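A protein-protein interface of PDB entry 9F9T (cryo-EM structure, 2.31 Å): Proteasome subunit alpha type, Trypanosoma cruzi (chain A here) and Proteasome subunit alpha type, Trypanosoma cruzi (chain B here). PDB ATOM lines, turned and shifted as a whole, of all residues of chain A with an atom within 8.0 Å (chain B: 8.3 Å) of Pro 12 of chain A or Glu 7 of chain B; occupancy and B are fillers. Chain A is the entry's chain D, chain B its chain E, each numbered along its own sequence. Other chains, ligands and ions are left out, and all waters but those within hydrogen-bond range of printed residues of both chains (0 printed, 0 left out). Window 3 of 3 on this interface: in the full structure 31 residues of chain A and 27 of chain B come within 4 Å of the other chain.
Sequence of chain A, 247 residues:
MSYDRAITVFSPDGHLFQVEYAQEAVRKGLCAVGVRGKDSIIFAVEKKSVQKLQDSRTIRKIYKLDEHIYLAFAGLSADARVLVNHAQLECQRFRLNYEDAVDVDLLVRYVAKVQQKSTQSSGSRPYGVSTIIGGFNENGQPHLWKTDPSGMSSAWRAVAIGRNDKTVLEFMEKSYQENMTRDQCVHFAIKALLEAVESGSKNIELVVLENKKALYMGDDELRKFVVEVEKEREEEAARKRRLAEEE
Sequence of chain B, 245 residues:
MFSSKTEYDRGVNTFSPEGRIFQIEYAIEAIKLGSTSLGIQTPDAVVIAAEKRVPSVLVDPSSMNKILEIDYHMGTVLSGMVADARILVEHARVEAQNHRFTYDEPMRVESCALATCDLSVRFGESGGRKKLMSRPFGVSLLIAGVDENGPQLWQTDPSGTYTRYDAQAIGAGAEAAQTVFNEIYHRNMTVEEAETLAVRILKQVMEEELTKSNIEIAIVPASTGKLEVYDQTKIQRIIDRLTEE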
ATOM      1  N   ALA A   6      27.087  14.600  22.636  1.00  0.00           N
ATOM      2  CA  ALA A   6      27.771  13.463  23.204  1.00  0.00           C
ATOM      3  C   ALA A   6      27.736  12.330  22.175  1.00  0.00           C
ATOM      4  O   ALA A   6      26.676  11.767  21.902  1.00  0.00           O
ATOM      5  CB  ALA A   6      27.092  13.107  24.514  1.00  0.00           C
ATOM      6  N   ILE A   7      28.913  11.990  21.635  1.00  0.00           N
ATOM      7  CA  ILE A   7      29.036  10.942  20.630  1.00  0.00           C
ATOM      8  C   ILE A   7      29.393   9.617  21.301  1.00  0.00           C
ATOM      9  O   ILE A   7      28.619   8.663  21.205  1.00  0.00           O
ATOM     10  CB  ILE A   7      30.015  11.401  19.528  1.00  0.00           C
ATOM     11  CG1 ILE A   7      29.441  12.618  18.774  1.00  0.00           C
ATOM     12  CG2 ILE A   7      30.358  10.251  18.585  1.00  0.00           C
ATOM     13  CD1 ILE A   7      30.468  13.506  18.080  1.00  0.00           C
ATOM     14  N   VAL A   9      29.203   7.216  24.115  1.00  0.00           N
ATOM     15  CA  VAL A   9      28.455   6.921  25.335  1.00  0.00           C
ATOM     16  C   VAL A   9      28.326   5.408  25.599  1.00  0.00           C
ATOM     17  O   VAL A   9      28.525   4.585  24.713  1.00  0.00           O
ATOM     18  CB  VAL A   9      27.066   7.567  25.268  1.00  0.00           C
ATOM     19  CG1 VAL A   9      27.210   9.063  25.101  1.00  0.00           C
ATOM     20  CG2 VAL A   9      26.205   6.949  24.167  1.00  0.00           C
ATOM     21  N   PHE A  10      28.000   5.067  26.846  1.00  0.00           N
ATOM     22  CA  PHE A  10      27.851   3.696  27.288  1.00  0.00           C
ATOM     23  C   PHE A  10      26.507   3.249  26.764  1.00  0.00           C
ATOM     24  O   PHE A  10      25.634   4.069  26.437  1.00  0.00           O
ATOM     25  CB  PHE A  10      27.930   3.518  28.815  1.00  0.00           C
ATOM     26  CG  PHE A  10      29.325   3.544  29.388  1.00  0.00           C
ATOM     27  CD1 PHE A  10      30.116   2.425  29.360  1.00  0.00           C
ATOM     28  CD2 PHE A  10      29.898   4.723  29.827  1.00  0.00           C
ATOM     29  CE1 PHE A  10      31.418   2.449  29.847  1.00  0.00           C
ATOM     30  CE2 PHE A  10      31.206   4.764  30.284  1.00  0.00           C
ATOM     31  CZ  PHE A  10      31.976   3.610  30.305  1.00  0.00           C
ATOM     32  N   SER A  11      26.408   1.935  26.635  1.00  0.00           N
ATOM     33  CA  SER A  11      25.162   1.339  26.215  1.00  0.00           C
ATOM     34  C   SER A  11      24.987   0.064  27.031  1.00  0.00           C
ATOM     35  O   SER A  11      25.899  -0.300  27.764  1.00  0.00           O
ATOM     36  CB  SER A  11      25.170   1.137  24.715  1.00  0.00           C
ATOM     37  OG  SER A  11      26.117   0.156  24.333  1.00  0.00           O
ATOM     38  N   PRO A  12      23.793  -0.566  27.020  1.00  0.00           N
ATOM     39  CA  PRO A  12      23.436  -1.610  27.986  1.00  0.00           C
ATOM     40  C   PRO A  12      24.238  -2.894  28.180  1.00  0.00           C
ATOM     41  O   PRO A  12      23.628  -3.959  28.240  1.00  0.00           O
ATOM     42  CB  PRO A  12      22.048  -2.025  27.504  1.00  0.00           C
ATOM     43  CG  PRO A  12      21.462  -0.756  26.937  1.00  0.00           C
ATOM     44  CD  PRO A  12      22.638  -0.144  26.218  1.00  0.00           C
ATOM     45  N   ASP A  13      25.554  -2.789  28.386  1.00  0.00           N
ATOM     46  CA  ASP A  13      26.348  -3.814  29.056  1.00  0.00           C
ATOM     47  C   ASP A  13      27.800  -3.357  29.191  1.00  0.00           C
ATOM     48  O   ASP A  13      28.708  -4.194  29.269  1.00  0.00           O
ATOM     49  CB  ASP A  13      26.444  -5.140  28.288  1.00  0.00           C
ATOM     50  CG  ASP A  13      25.140  -5.795  27.842  1.00  0.00           C
ATOM     51  OD1 ASP A  13      24.445  -6.400  28.699  1.00  0.00           O
ATOM     52  OD2 ASP A  13      24.837  -5.719  26.624  1.00  0.00           O
ATOM     53  N   GLY A  14      28.030  -2.029  29.217  1.00  0.00           N
ATOM     54  CA  GLY A  14      29.357  -1.473  29.462  1.00  0.00           C
ATOM     55  C   GLY A  14      30.162  -1.292  28.176  1.00  0.00           C
ATOM     56  O   GLY A  14      31.383  -1.116  28.214  1.00  0.00           O
ATOM     57  N   HIS A  15      29.431  -1.318  27.058  1.00  0.00           N
ATOM     58  CA  HIS A  15      29.990  -1.169  25.731  1.00  0.00           C
ATOM     59  C   HIS A  15      30.036   0.314  25.363  1.00  0.00           C
ATOM     60  O   HIS A  15      29.017   1.007  25.492  1.00  0.00           O
ATOM     61  CB  HIS A  15      29.159  -2.005  24.743  1.00  0.00           C
ATOM     62  CG  HIS A  15      29.411  -3.483  24.859  1.00  0.00           C
ATOM     63  ND1 HIS A  15      28.420  -4.431  24.703  1.00  0.00           N
ATOM     64  CD2 HIS A  15      30.556  -4.171  25.104  1.00  0.00           C
ATOM     65  CE1 HIS A  15      28.954  -5.638  24.855  1.00  0.00           C
ATOM     66  NE2 HIS A  15      30.248  -5.504  25.095  1.00  0.00           N
ATOM     67  N   LEU A  16      31.224   0.783  24.931  1.00  0.00           N
ATOM     68  CA  LEU A  16      31.376   2.023  24.170  1.00  0.00           C
ATOM     69  C   LEU A  16      31.505   1.710  22.672  1.00  0.00           C
ATOM     70  O   LEU A  16      32.626   1.450  22.206  1.00  0.00           O
ATOM     71  CB  LEU A  16      32.666   2.737  24.594  1.00  0.00           C
ATOM     72  CG  LEU A  16      32.796   3.146  26.045  1.00  0.00           C
ATOM     73  CD1 LEU A  16      34.127   3.851  26.272  1.00  0.00           C
ATOM     74  CD2 LEU A  16      31.643   4.058  26.434  1.00  0.00           C
ATOM     75  N   PHE A  17      30.401   1.821  21.920  1.00  0.00           N
ATOM     76  CA  PHE A  17      30.364   1.353  20.541  1.00  0.00           C
ATOM     77  C   PHE A  17      31.274   2.199  19.665  1.00  0.00           C
ATOM     78  O   PHE A  17      31.982   1.653  18.819  1.00  0.00           O
ATOM     79  CB  PHE A  17      28.952   1.354  19.940  1.00  0.00           C
ATOM     80  CG  PHE A  17      28.019   0.294  20.476  1.00  0.00           C
ATOM     81  CD1 PHE A  17      28.471  -0.989  20.755  1.00  0.00           C
ATOM     82  CD2 PHE A  17      26.664   0.553  20.631  1.00  0.00           C
ATOM     83  CE1 PHE A  17      27.614  -1.969  21.234  1.00  0.00           C
ATOM     84  CE2 PHE A  17      25.796  -0.431  21.094  1.00  0.00           C
ATOM     85  CZ  PHE A  17      26.279  -1.679  21.419  1.00  0.00           C
ATOM     86  N   TYR A  21      33.948   0.186  17.154  1.00  0.00           N
ATOM     87  CA  TYR A  21      33.882   0.361  15.722  1.00  0.00           C
ATOM     88  C   TYR A  21      35.151   1.053  15.248  1.00  0.00           C
ATOM     89  O   TYR A  21      35.609   0.797  14.155  1.00  0.00           O
ATOM     90  CB  TYR A  21      32.693   1.252  15.334  1.00  0.00           C
ATOM     91  CG  TYR A  21      31.280   0.865  15.748  1.00  0.00           C
ATOM     92  CD1 TYR A  21      30.902  -0.440  16.032  1.00  0.00           C
ATOM     93  CD2 TYR A  21      30.298   1.860  15.824  1.00  0.00           C
ATOM     94  CE1 TYR A  21      29.578  -0.733  16.387  1.00  0.00           C
ATOM     95  CE2 TYR A  21      28.988   1.580  16.189  1.00  0.00           C
ATOM     96  CZ  TYR A  21      28.623   0.271  16.463  1.00  0.00           C
ATOM     97  OH  TYR A  21      27.318   0.045  16.803  1.00  0.00           O
ATOM     98  N   GLU B   7      20.482   3.813  21.799  1.00  0.00           N
ATOM     99  CA  GLU B   7      21.810   4.308  22.266  1.00  0.00           C
ATOM    100  C   GLU B   7      21.816   5.836  22.253  1.00  0.00           C
ATOM    101  O   GLU B   7      22.236   6.465  23.219  1.00  0.00           O
ATOM    102  CB  GLU B   7      22.928   3.687  21.419  1.00  0.00           C
ATOM    103  CG  GLU B   7      23.309   2.269  21.844  1.00  0.00           C
ATOM    104  CD  GLU B   7      22.200   1.348  22.349  1.00  0.00           C
ATOM    105  OE1 GLU B   7      21.711   1.556  23.486  1.00  0.00           O
ATOM    106  OE2 GLU B   7      21.825   0.411  21.611  1.00  0.00           O
ATOM    107  N   TYR B   8      21.323   6.418  21.154  1.00  0.00           N
ATOM    108  CA  TYR B   8      21.136   7.855  21.042  1.00  0.00           C
ATOM    109  C   TYR B   8      19.658   8.222  21.249  1.00  0.00           C
ATOM    110  O   TYR B   8      19.326   9.407  21.307  1.00  0.00           O
ATOM    111  CB  TYR B   8      21.730   8.278  19.691  1.00  0.00           C
ATOM    112  CG  TYR B   8      23.249   8.191  19.544  1.00  0.00           C
ATOM    113  CD1 TYR B   8      24.110   8.722  20.509  1.00  0.00           C
ATOM    114  CD2 TYR B   8      23.831   7.627  18.408  1.00  0.00           C
ATOM    115  CE1 TYR B   8      25.489   8.669  20.363  1.00  0.00           C
ATOM    116  CE2 TYR B   8      25.210   7.570  18.252  1.00  0.00           C
ATOM    117  CZ  TYR B   8      26.039   8.095  19.229  1.00  0.00           C
ATOM    118  OH  TYR B   8      27.391   8.041  19.071  1.00  0.00           O
ATOM    119  N   ASP B   9      18.790   7.204  21.404  1.00  0.00           N
ATOM    120  CA  ASP B   9      17.351   7.369  21.606  1.00  0.00           C
ATOM    121  C   ASP B   9      17.082   8.161  22.894  1.00  0.00           C
ATOM    122  O   ASP B   9      16.128   8.940  22.956  1.00  0.00           O
ATOM    123  CB  ASP B   9      16.644   6.003  21.639  1.00  0.00           C
ATOM    124  CG  ASP B   9      15.436   5.884  20.723  1.00  0.00           C
ATOM    125  OD1 ASP B   9      15.647   5.719  19.500  1.00  0.00           O
ATOM    126  OD2 ASP B   9      14.295   5.956  21.235  1.00  0.00           O
ATOM    127  N   ARG B  10      17.928   7.943  23.920  1.00  0.00           N
ATOM    128  CA  ARG B  10      17.845   8.646  25.194  1.00  0.00           C
ATOM    129  C   ARG B  10      19.217   9.208  25.570  1.00  0.00           C
ATOM    130  O   ARG B  10      20.265   8.607  25.335  1.00  0.00           O
ATOM    131  CB  ARG B  10      17.339   7.732  26.313  1.00  0.00           C
ATOM    132  CG  ARG B  10      18.310   6.614  26.673  1.00  0.00           C
ATOM    133  CD  ARG B  10      17.766   5.564  27.624  1.00  0.00           C
ATOM    134  NE  ARG B  10      16.335   5.291  27.502  1.00  0.00           N
ATOM    135  CZ  ARG B  10      15.782   4.129  27.822  1.00  0.00           C
ATOM    136  NH1 ARG B  10      16.555   3.069  27.978  1.00  0.00           N
ATOM    137  NH2 ARG B  10      14.469   4.019  27.954  1.00  0.00           N
ATOM    138  N   GLY B  11      19.180  10.366  26.219  1.00  0.00           N
ATOM    139  CA  GLY B  11      20.352  11.190  26.416  1.00  0.00           C
ATOM    140  C   GLY B  11      21.204  10.756  27.598  1.00  0.00           C
ATOM    141  O   GLY B  11      20.878   9.844  28.358  1.00  0.00           O
ATOM    142  N   VAL B  12      22.285  11.512  27.753  1.00  0.00           N
ATOM    143  CA  VAL B  12      23.350  11.220  28.687  1.00  0.00           C
ATOM    144  C   VAL B  12      22.909  11.445  30.134  1.00  0.00           C
ATOM    145  O   VAL B  12      23.492  10.874  31.052  1.00  0.00           O
ATOM    146  CB  VAL B  12      24.546  12.080  28.261  1.00  0.00           C
ATOM    147  CG1 VAL B  12      25.363  12.620  29.427  1.00  0.00           C
ATOM    148  CG2 VAL B  12      25.416  11.291  27.285  1.00  0.00           C
ATOM    149  N   PHE B  22      21.044   6.154  33.522  1.00  0.00           N
ATOM    150  CA  PHE B  22      21.422   5.027  32.684  1.00  0.00           C
ATOM    151  C   PHE B  22      22.932   5.014  32.453  1.00  0.00           C
ATOM    152  O   PHE B  22      23.587   4.001  32.676  1.00  0.00           O
ATOM    153  CB  PHE B  22      20.611   5.060  31.387  1.00  0.00           C
ATOM    154  CG  PHE B  22      19.194   4.552  31.496  1.00  0.00           C
ATOM    155  CD1 PHE B  22      18.938   3.258  31.872  1.00  0.00           C
ATOM    156  CD2 PHE B  22      18.115   5.388  31.252  1.00  0.00           C
ATOM    157  CE1 PHE B  22      17.637   2.788  31.972  1.00  0.00           C
ATOM    158  CE2 PHE B  22      16.804   4.922  31.333  1.00  0.00           C
ATOM    159  CZ  PHE B  22      16.566   3.624  31.694  1.00  0.00           C
ATOM    160  N   GLN B  23      23.489   6.163  32.056  1.00  0.00           N
ATOM    161  CA  GLN B  23      24.913   6.184  31.788  1.00  0.00           C
ATOM    162  C   GLN B  23      25.701   5.561  32.945  1.00  0.00           C
ATOM    163  O   GLN B  23      26.679   4.861  32.684  1.00  0.00           O
ATOM    164  CB  GLN B  23      25.435   7.584  31.404  1.00  0.00           C
ATOM    165  CG  GLN B  23      25.135   7.997  29.948  1.00  0.00           C
ATOM    166  CD  GLN B  23      25.789   7.047  28.963  1.00  0.00           C
ATOM    167  OE1 GLN B  23      27.016   6.972  28.890  1.00  0.00           O
ATOM    168  NE2 GLN B  23      24.985   6.240  28.288  1.00  0.00           N
ATOM    169  N   GLU B  25      24.603   3.313  35.432  1.00  0.00           N
ATOM    170  CA  GLU B  25      24.417   1.880  35.526  1.00  0.00           C
ATOM    171  C   GLU B  25      25.334   1.162  34.543  1.00  0.00           C
ATOM    172  O   GLU B  25      26.058   0.233  34.918  1.00  0.00           O
ATOM    173  CB  GLU B  25      22.938   1.552  35.367  1.00  0.00           C
ATOM    174  CG  GLU B  25      22.150   2.030  36.582  1.00  0.00           C
ATOM    175  CD  GLU B  25      22.848   1.774  37.924  1.00  0.00           C
ATOM    176  OE1 GLU B  25      23.029   0.579  38.281  1.00  0.00           O
ATOM    177  OE2 GLU B  25      23.250   2.766  38.611  1.00  0.00           O
ATOM    178  N   TYR B  26      25.328   1.610  33.281  1.00  0.00           N
ATOM    179  CA  TYR B  26      26.067   0.896  32.251  1.00  0.00           C
ATOM    180  C   TYR B  26      27.555   0.981  32.553  1.00  0.00           C
ATOM    181  O   TYR B  26      28.262   0.026  32.327  1.00  0.00           O
ATOM    182  CB  TYR B  26      25.783   1.400  30.831  1.00  0.00           C
ATOM    183  CG  TYR B  26      24.321   1.428  30.376  1.00  0.00           C
ATOM    184  CD1 TYR B  26      23.396   0.446  30.753  1.00  0.00           C
ATOM    185  CD2 TYR B  26      23.864   2.495  29.572  1.00  0.00           C
ATOM    186  CE1 TYR B  26      22.055   0.543  30.361  1.00  0.00           C
ATOM    187  CE2 TYR B  26      22.545   2.583  29.166  1.00  0.00           C
ATOM    188  CZ  TYR B  26      21.632   1.620  29.574  1.00  0.00           C
ATOM    189  OH  TYR B  26      20.359   1.786  29.076  1.00  0.00           O
ATOM    190  N   ALA B  27      28.034   2.107  33.100  1.00  0.00           N
ATOM    191  CA  ALA B  27      29.462   2.238  33.395  1.00  0.00           C
ATOM    192  C   ALA B  27      29.920   1.244  34.462  1.00  0.00           C
ATOM    193  O   ALA B  27      31.004   0.715  34.341  1.00  0.00           O
ATOM    194  CB  ALA B  27      29.809   3.653  33.790  1.00  0.00           C
ATOM    195  N   GLU B  29      28.510  -1.700  34.961  1.00  0.00           N
ATOM    196  CA  GLU B  29      28.584  -2.994  34.280  1.00  0.00           C
ATOM    197  C   GLU B  29      29.962  -3.179  33.641  1.00  0.00           C
ATOM    198  O   GLU B  29      30.544  -4.251  33.660  1.00  0.00           O
ATOM    199  CB  GLU B  29      27.524  -3.144  33.184  1.00  0.00           C
ATOM    200  CG  GLU B  29      26.088  -3.124  33.681  1.00  0.00           C
ATOM    201  CD  GLU B  29      25.584  -4.436  34.259  1.00  0.00           C
ATOM    202  OE1 GLU B  29      25.614  -4.580  35.510  1.00  0.00           O
ATOM    203  OE2 GLU B  29      25.139  -5.303  33.462  1.00  0.00           O
ATOM    204  N   ALA B  30      30.486  -2.099  33.084  1.00  0.00           N
ATOM    205  CA  ALA B  30      31.784  -2.104  32.452  1.00  0.00           C
ATOM    206  C   ALA B  30      32.872  -2.544  33.401  1.00  0.00           C
ATOM    207  O   ALA B  30      33.820  -3.179  32.965  1.00  0.00           O
ATOM    208  CB  ALA B  30      32.101  -0.723  31.939  1.00  0.00           C
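The backbone carbonyl oxygen (O) of Phe 10 of chain A lies within hydrogen-bond range of the side-chain amide nitrogen (NE2) of Gln 23 of chain B. The side-chain hydroxyl (OH) of Tyr 8 of chain B is in hydrogen-bond range of the backbone carbonyl oxygen (O) of Ile 7 of chain A, at 2.5 Å.
CG2 of Val 12 of chain B touches CG1 of Val 9 of chain A (3.6 Å). Val 9 of chain A touches Gln 23 of chain B. Phe 10 of chain A touches Tyr 26 of chain B. Phe 10 of chain A touches Ala 27 of chain B. Phe 10 of chain A touches Ala 30 of chain B (CE1 to CB, 3.9 Å). Ser 11 of chain A touches Tyr 26 of chain B (O to CG, 3.5 Å). Glu 7 of chain B touches Pro 12 of chain A (OE1 to CD, 3.3 Å). CA of Gly 14 of chain A touches O of Tyr 26 of chain B, at 3.4 Å. Gly 14 of chain A touches Ala 30 of chain B. CG of Glu 7 of chain B touches CE2 of Phe 17 of chain A, at 3.7 Å.
Hydrophobic or aromatic side chains of chain A within 4 Å of the printed part of chain B: Ala 6, Ile 7, Val 9, Phe 10, Pro 12 and Phe 17. Hydrophobic or aromatic side chains of chain B within 4 Å of the printed part of chain A: Tyr 8, Val 12, Tyr 26, Ala 27 and Ala 30. Along chain B the printed residues that touch a printed residue of chain A span positions 7 to 30.
Of the printed residues of chain B, Phe 10 of chain A touches Gln 23 (2.9 Å), Tyr 26 (3.6 Å), Ala 27 (3.9 Å) and Ala 30 (3.9 Å). Of chain B, only Glu 7 and Tyr 26 come within 4 Å of Pro 12 of chain A. Gly 11 of chain B touches none of the printed residues of chain A. Of the printed residues of chain A, Ala 30 of chain B touches Phe 10 and Gly 14. The nearest residue of chain B that does not touch Pro 12 of chain A is Glu 29 of chain B (5.6 Å).
OG of Ser 11 of chain A sits at hydrogen-bond distance from O of His 15 of chain A (3.2 Å).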
